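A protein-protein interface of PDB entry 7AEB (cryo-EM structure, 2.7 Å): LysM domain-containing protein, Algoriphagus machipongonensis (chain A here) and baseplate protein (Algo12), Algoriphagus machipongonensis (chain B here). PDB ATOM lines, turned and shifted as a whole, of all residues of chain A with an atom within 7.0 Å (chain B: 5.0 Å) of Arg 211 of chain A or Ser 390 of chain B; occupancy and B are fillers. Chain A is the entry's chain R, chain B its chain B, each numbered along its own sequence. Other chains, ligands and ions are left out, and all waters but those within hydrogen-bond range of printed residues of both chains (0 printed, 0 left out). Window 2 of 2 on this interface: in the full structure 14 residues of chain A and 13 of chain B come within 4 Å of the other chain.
Among the printed residues, pairs that only touch across the chains: Phe 210 of chain A with Asp 63 of chain B (3.3 Å), Arg 211 of chain A with Tyr 59 of chain B (3.3 Å) and Arg 212 of chain A with Ser 390 of chain B (3.6 Å).
The side-chain amino group (NZ) of Lys 214 of chain A sits at hydrogen-bond distance from the backbone carbonyl oxygen (O) of Arg 212 of chain A (3.3 Å).
Arg 211 of chain A touches just these residues of chain B: Tyr 59, Asp 63, Ser 390 and Glu 395.
Printed residues of chain A within 4 Å of Ser 390 of chain B: Arg 211 and Arg 212.
Printed residues of chain B within 4 Å of Thr 208 of chain A: Asp 63.
Of the printed residues of chain A, Glu 395 of chain B touches Arg 211.
The nearest residue of chain A that does not touch Ser 390 of chain B is Asn 209 of chain A (4.1 Å).
The nearest printed residue of chain B that does not touch Thr 208 of chain A is Glu 388 of chain B (5.7 Å).
OD2 of Asp 63 of chain B lies within salt-bridge range of NH1 of Arg 211 of chain A, at 3.1 Å.
O of Ser 390 of chain B lies within hydrogen-bond range of NH2 of Arg 211 of chain A (2.8 Å).
OE2 of Glu 395 of chain B lies within salt-bridge range of NE of Arg 211 of chain A, at 3.7 Å.
The backbone carbonyl oxygen (O) of Thr 208 of chain A sits close to the side-chain carboxylate (OD1) of Asp 63 of chain B.
Along chain B the printed residues that touch a printed residue of chain A span positions 59 to 395.
Of the 10 printed residues of chain A, 4 touch a printed residue of chain B.
Hydrophobic or aromatic side chains of chain A that line the printed part of chain B: Phe 210.
Among the printed residues, Asp or Glu carboxylates within 4 Å of a Lys or Arg side-chain nitrogen of the other chain: Arg 211 of chain A with Asp 63 of chain B (3.1 Å) and Arg 211 of chain A with Glu 395 of chain B (3.7 Å).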
ATOM      1  N   ASP A 182      -9.631  16.503  10.232  1.00  0.00           N
ATOM      2  CA  ASP A 182      -9.108  17.394  11.255  1.00  0.00           C
ATOM      3  C   ASP A 182      -7.960  18.234  10.714  1.00  0.00           C
ATOM      4  O   ASP A 182      -7.165  17.781   9.890  1.00  0.00           O
ATOM      5  CB  ASP A 182      -8.613  16.601  12.464  1.00  0.00           C
ATOM      6  CG  ASP A 182      -9.738  16.054  13.310  1.00  0.00           C
ATOM      7  OD1 ASP A 182     -10.890  16.497  13.131  1.00  0.00           O
ATOM      8  OD2 ASP A 182      -9.467  15.180  14.162  1.00  0.00           O
ATOM      9  N   THR A 183      -7.878  19.471  11.196  1.00  0.00           N
ATOM     10  CA  THR A 183      -6.734  20.335  10.950  1.00  0.00           C
ATOM     11  C   THR A 183      -6.198  20.800  12.290  1.00  0.00           C
ATOM     12  O   THR A 183      -6.924  20.829  13.284  1.00  0.00           O
ATOM     13  CB  THR A 183      -7.088  21.548  10.082  1.00  0.00           C
ATOM     14  OG1 THR A 183      -8.189  22.248  10.664  1.00  0.00           O
ATOM     15  CG2 THR A 183      -7.468  21.120   8.679  1.00  0.00           C
ATOM     16  N   LEU A 184      -4.917  21.149  12.318  1.00  0.00           N
ATOM     17  CA  LEU A 184      -4.299  21.595  13.563  1.00  0.00           C
ATOM     18  C   LEU A 184      -4.799  22.956  14.073  1.00  0.00           C
ATOM     19  O   LEU A 184      -4.996  23.076  15.292  1.00  0.00           O
ATOM     20  CB  LEU A 184      -2.772  21.577  13.429  1.00  0.00           C
ATOM     21  CG  LEU A 184      -1.988  21.719  14.735  1.00  0.00           C
ATOM     22  CD1 LEU A 184      -2.142  20.491  15.595  1.00  0.00           C
ATOM     23  CD2 LEU A 184      -0.532  22.009  14.495  1.00  0.00           C
ATOM     24  N   THR A 208       6.747  17.949  11.949  1.00  0.00           N
ATOM     25  CA  THR A 208       7.350  18.835  10.968  1.00  0.00           C
ATOM     26  C   THR A 208       6.365  19.166   9.861  1.00  0.00           C
ATOM     27  O   THR A 208       6.205  20.332   9.492  1.00  0.00           O
ATOM     28  CB  THR A 208       8.625  18.212  10.382  1.00  0.00           C
ATOM     29  OG1 THR A 208       8.279  17.089   9.566  1.00  0.00           O
ATOM     30  CG2 THR A 208       9.555  17.761  11.491  1.00  0.00           C
ATOM     31  N   ASN A 209       5.683  18.152   9.336  1.00  0.00           N
ATOM     32  CA  ASN A 209       4.635  18.349   8.341  1.00  0.00           C
ATOM     33  C   ASN A 209       3.271  18.373   9.036  1.00  0.00           C
ATOM     34  O   ASN A 209       2.466  17.448   8.939  1.00  0.00           O
ATOM     35  CB  ASN A 209       4.705  17.259   7.279  1.00  0.00           C
ATOM     36  CG  ASN A 209       4.068  17.681   5.968  1.00  0.00           C
ATOM     37  OD1 ASN A 209       4.565  18.575   5.284  1.00  0.00           O
ATOM     38  ND2 ASN A 209       2.969  17.032   5.607  1.00  0.00           N
ATOM     39  N   PHE A 210       3.013  19.475   9.741  1.00  0.00           N
ATOM     40  CA  PHE A 210       1.757  19.600  10.470  1.00  0.00           C
ATOM     41  C   PHE A 210       0.587  20.012   9.587  1.00  0.00           C
ATOM     42  O   PHE A 210      -0.547  20.022  10.068  1.00  0.00           O
ATOM     43  CB  PHE A 210       1.900  20.584  11.643  1.00  0.00           C
ATOM     44  CG  PHE A 210       2.347  21.977  11.255  1.00  0.00           C
ATOM     45  CD1 PHE A 210       1.425  22.958  10.922  1.00  0.00           C
ATOM     46  CD2 PHE A 210       3.688  22.314  11.282  1.00  0.00           C
ATOM     47  CE1 PHE A 210       1.836  24.221  10.579  1.00  0.00           C
ATOM     48  CE2 PHE A 210       4.101  23.583  10.947  1.00  0.00           C
ATOM     49  CZ  PHE A 210       3.172  24.537  10.597  1.00  0.00           C
ATOM     50  N   ARG A 211       0.820  20.354   8.321  1.00  0.00           N
ATOM     51  CA  ARG A 211      -0.280  20.800   7.476  1.00  0.00           C
ATOM     52  C   ARG A 211      -1.038  19.641   6.864  1.00  0.00           C
ATOM     53  O   ARG A 211      -2.104  19.851   6.276  1.00  0.00           O
ATOM     54  CB  ARG A 211       0.241  21.746   6.396  1.00  0.00           C
ATOM     55  CG  ARG A 211       0.445  23.158   6.911  1.00  0.00           C
ATOM     56  CD  ARG A 211       1.334  23.989   6.014  1.00  0.00           C
ATOM     57  NE  ARG A 211       1.020  23.783   4.609  1.00  0.00           N
ATOM     58  CZ  ARG A 211       1.894  23.916   3.622  1.00  0.00           C
ATOM     59  NH1 ARG A 211       3.142  24.259   3.883  1.00  0.00           N
ATOM     60  NH2 ARG A 211       1.520  23.705   2.374  1.00  0.00           N
ATOM     61  N   ARG A 212      -0.517  18.439   7.064  1.00  0.00           N
ATOM     62  CA  ARG A 212      -1.176  17.203   6.693  1.00  0.00           C
ATOM     63  C   ARG A 212      -1.025  16.266   7.886  1.00  0.00           C
ATOM     64  O   ARG A 212       0.086  15.813   8.172  1.00  0.00           O
ATOM     65  CB  ARG A 212      -0.527  16.601   5.449  1.00  0.00           C
ATOM     66  CG  ARG A 212      -0.480  17.532   4.248  1.00  0.00           C
ATOM     67  CD  ARG A 212      -1.869  17.789   3.693  1.00  0.00           C
ATOM     68  NE  ARG A 212      -2.472  16.579   3.147  1.00  0.00           N
ATOM     69  CZ  ARG A 212      -3.656  16.538   2.544  1.00  0.00           C
ATOM     70  NH1 ARG A 212      -4.371  17.646   2.409  1.00  0.00           N
ATOM     71  NH2 ARG A 212      -4.125  15.390   2.075  1.00  0.00           N
ATOM     72  N   LEU A 213      -2.112  15.967   8.593  1.00  0.00           N
ATOM     73  CA  LEU A 213      -2.033  15.024   9.700  1.00  0.00           C
ATOM     74  C   LEU A 213      -2.505  13.647   9.254  1.00  0.00           C
ATOM     75  O   LEU A 213      -3.467  13.524   8.495  1.00  0.00           O
ATOM     76  CB  LEU A 213      -2.857  15.499  10.898  1.00  0.00           C
ATOM     77  CG  LEU A 213      -2.610  16.924  11.394  1.00  0.00           C
ATOM     78  CD1 LEU A 213      -3.634  17.313  12.445  1.00  0.00           C
ATOM     79  CD2 LEU A 213      -1.206  17.070  11.940  1.00  0.00           C
ATOM     80  N   LYS A 214      -1.810  12.619   9.730  1.00  0.00           N
ATOM     81  CA  LYS A 214      -2.165  11.234   9.466  1.00  0.00           C
ATOM     82  C   LYS A 214      -3.193  10.758  10.482  1.00  0.00           C
ATOM     83  O   LYS A 214      -3.128  11.107  11.663  1.00  0.00           O
ATOM     84  CB  LYS A 214      -0.927  10.341   9.510  1.00  0.00           C
ATOM     85  CG  LYS A 214       0.249  10.884   8.720  1.00  0.00           C
ATOM     86  CD  LYS A 214      -0.051  10.893   7.229  1.00  0.00           C
ATOM     87  CE  LYS A 214       1.020  11.635   6.439  1.00  0.00           C
ATOM     88  NZ  LYS A 214       0.743  13.095   6.331  1.00  0.00           N
ATOM     89  N   TYR B  59       0.456  31.378   6.194  1.00  0.00           N
ATOM     90  CA  TYR B  59       0.488  30.091   6.870  1.00  0.00           C
ATOM     91  C   TYR B  59       1.650  29.244   6.361  1.00  0.00           C
ATOM     92  O   TYR B  59       2.413  28.680   7.152  1.00  0.00           O
ATOM     93  CB  TYR B  59      -0.876  29.439   6.682  1.00  0.00           C
ATOM     94  CG  TYR B  59      -1.091  28.111   7.272  1.00  0.00           C
ATOM     95  CD1 TYR B  59      -1.149  27.954   8.631  1.00  0.00           C
ATOM     96  CD2 TYR B  59      -1.321  27.034   6.468  1.00  0.00           C
ATOM     97  CE1 TYR B  59      -1.399  26.740   9.175  1.00  0.00           C
ATOM     98  CE2 TYR B  59      -1.581  25.818   7.009  1.00  0.00           C
ATOM     99  CZ  TYR B  59      -1.618  25.674   8.362  1.00  0.00           C
ATOM    100  OH  TYR B  59      -1.885  24.453   8.906  1.00  0.00           O
ATOM    101  N   ALA B  60       1.810  29.174   5.036  1.00  0.00           N
ATOM    102  CA  ALA B  60       2.907  28.431   4.422  1.00  0.00           C
ATOM    103  C   ALA B  60       4.281  28.951   4.844  1.00  0.00           C
ATOM    104  O   ALA B  60       5.211  28.161   5.040  1.00  0.00           O
ATOM    105  CB  ALA B  60       2.781  28.499   2.916  1.00  0.00           C
ATOM    106  N   ASP B  63       5.343  27.610   8.253  1.00  0.00           N
ATOM    107  CA  ASP B  63       5.808  26.228   8.145  1.00  0.00           C
ATOM    108  C   ASP B  63       7.270  26.170   7.729  1.00  0.00           C
ATOM    109  O   ASP B  63       8.063  25.428   8.317  1.00  0.00           O
ATOM    110  CB  ASP B  63       4.936  25.463   7.144  1.00  0.00           C
ATOM    111  CG  ASP B  63       5.291  23.991   7.000  1.00  0.00           C
ATOM    112  OD1 ASP B  63       5.447  23.321   7.996  1.00  0.00           O
ATOM    113  OD2 ASP B  63       5.334  23.511   5.882  1.00  0.00           O
ATOM    114  N   GLU B 388      10.221  17.645   2.459  1.00  0.00           N
ATOM    115  CA  GLU B 388       8.850  17.308   2.058  1.00  0.00           C
ATOM    116  C   GLU B 388       7.956  18.529   1.927  1.00  0.00           C
ATOM    117  O   GLU B 388       7.876  19.335   2.846  1.00  0.00           O
ATOM    118  CB  GLU B 388       8.230  16.323   3.042  1.00  0.00           C
ATOM    119  CG  GLU B 388       6.892  15.768   2.580  1.00  0.00           C
ATOM    120  CD  GLU B 388       6.239  14.842   3.562  1.00  0.00           C
ATOM    121  OE1 GLU B 388       6.775  14.625   4.633  1.00  0.00           O
ATOM    122  OE2 GLU B 388       5.239  14.249   3.202  1.00  0.00           O
ATOM    123  N   TYR B 389       7.234  18.654   0.811  1.00  0.00           N
ATOM    124  CA  TYR B 389       6.390  19.829   0.584  1.00  0.00           C
ATOM    125  C   TYR B 389       5.007  19.480   0.059  1.00  0.00           C
ATOM    126  O   TYR B 389       4.882  18.661  -0.851  1.00  0.00           O
ATOM    127  CB  TYR B 389       7.068  20.772  -0.413  1.00  0.00           C
ATOM    128  CG  TYR B 389       6.234  21.958  -0.829  1.00  0.00           C
ATOM    129  CD1 TYR B 389       6.106  23.019   0.004  1.00  0.00           C
ATOM    130  CD2 TYR B 389       5.593  21.993  -2.058  1.00  0.00           C
ATOM    131  CE1 TYR B 389       5.364  24.093  -0.346  1.00  0.00           C
ATOM    132  CE2 TYR B 389       4.836  23.081  -2.416  1.00  0.00           C
ATOM    133  CZ  TYR B 389       4.730  24.127  -1.554  1.00  0.00           C
ATOM    134  OH  TYR B 389       3.982  25.232  -1.862  1.00  0.00           O
ATOM    135  N   SER B 390       3.978  20.134   0.605  1.00  0.00           N
ATOM    136  CA  SER B 390       2.605  19.974   0.142  1.00  0.00           C
ATOM    137  C   SER B 390       2.096  21.270  -0.473  1.00  0.00           C
ATOM    138  O   SER B 390       2.317  22.343   0.081  1.00  0.00           O
ATOM    139  CB  SER B 390       1.685  19.617   1.290  1.00  0.00           C
ATOM    140  OG  SER B 390       2.024  18.387   1.855  1.00  0.00           O
ATOM    141  N   SER B 391       1.374  21.151  -1.582  1.00  0.00           N
ATOM    142  CA  SER B 391       0.821  22.291  -2.311  1.00  0.00           C
ATOM    143  C   SER B 391      -0.141  23.152  -1.515  1.00  0.00           C
ATOM    144  O   SER B 391      -0.993  22.654  -0.778  1.00  0.00           O
ATOM    145  CB  SER B 391       0.108  21.798  -3.544  1.00  0.00           C
ATOM    146  OG  SER B 391      -0.577  22.848  -4.151  1.00  0.00           O
ATOM    147  N   ILE B 392      -0.055  24.469  -1.727  1.00  0.00           N
ATOM    148  CA  ILE B 392      -0.926  25.414  -1.028  1.00  0.00           C
ATOM    149  C   ILE B 392      -2.342  25.366  -1.549  1.00  0.00           C
ATOM    150  O   ILE B 392      -3.250  25.945  -0.964  1.00  0.00           O
ATOM    151  CB  ILE B 392      -0.415  26.865  -1.121  1.00  0.00           C
ATOM    152  CG1 ILE B 392      -0.460  27.371  -2.588  1.00  0.00           C
ATOM    153  CG2 ILE B 392       0.971  26.948  -0.522  1.00  0.00           C
ATOM    154  CD1 ILE B 392      -0.154  28.844  -2.791  1.00  0.00           C
ATOM    155  N   GLU B 395      -5.219  24.208   0.722  1.00  0.00           N
ATOM    156  CA  GLU B 395      -5.660  25.055   1.807  1.00  0.00           C
ATOM    157  C   GLU B 395      -6.904  25.861   1.455  1.00  0.00           C
ATOM    158  O   GLU B 395      -7.395  26.619   2.288  1.00  0.00           O
ATOM    159  CB  GLU B 395      -4.546  26.021   2.188  1.00  0.00           C
ATOM    160  CG  GLU B 395      -3.243  25.378   2.647  1.00  0.00           C
ATOM    161  CD  GLU B 395      -3.374  24.642   3.908  1.00  0.00           C
ATOM    162  OE1 GLU B 395      -4.151  25.061   4.736  1.00  0.00           O
ATOM    163  OE2 GLU B 395      -2.687  23.658   4.088  1.00  0.00           O
ATOM    164  N   ASP B 430       3.811  28.145  -5.693  1.00  0.00           N
ATOM    165  CA  ASP B 430       4.241  26.866  -5.169  1.00  0.00           C
ATOM    166  C   ASP B 430       5.608  26.498  -5.668  1.00  0.00           C
ATOM    167  O   ASP B 430       6.372  25.887  -4.922  1.00  0.00           O
ATOM    168  CB  ASP B 430       3.354  25.700  -5.586  1.00  0.00           C
ATOM    169  CG  ASP B 430       2.032  25.602  -4.926  1.00  0.00           C
ATOM    170  OD1 ASP B 430       1.990  25.329  -3.718  1.00  0.00           O
ATOM    171  OD2 ASP B 430       1.034  25.724  -5.631  1.00  0.00           O
ATOM    172  N   ASP B 464       1.375  16.647  -6.095  1.00  0.00           N
ATOM    173  CA  ASP B 464       0.168  16.459  -5.308  1.00  0.00           C
ATOM    174  C   ASP B 464      -0.979  17.315  -5.832  1.00  0.00           C
ATOM    175  O   ASP B 464      -1.933  17.625  -5.114  1.00  0.00           O
ATOM    176  CB  ASP B 464       0.466  16.724  -3.841  1.00  0.00           C
ATOM    177  CG  ASP B 464       1.033  18.068  -3.623  1.00  0.00           C
ATOM    178  OD1 ASP B 464       1.632  18.592  -4.553  1.00  0.00           O
ATOM    179  OD2 ASP B 464       0.876  18.604  -2.537  1.00  0.00           O
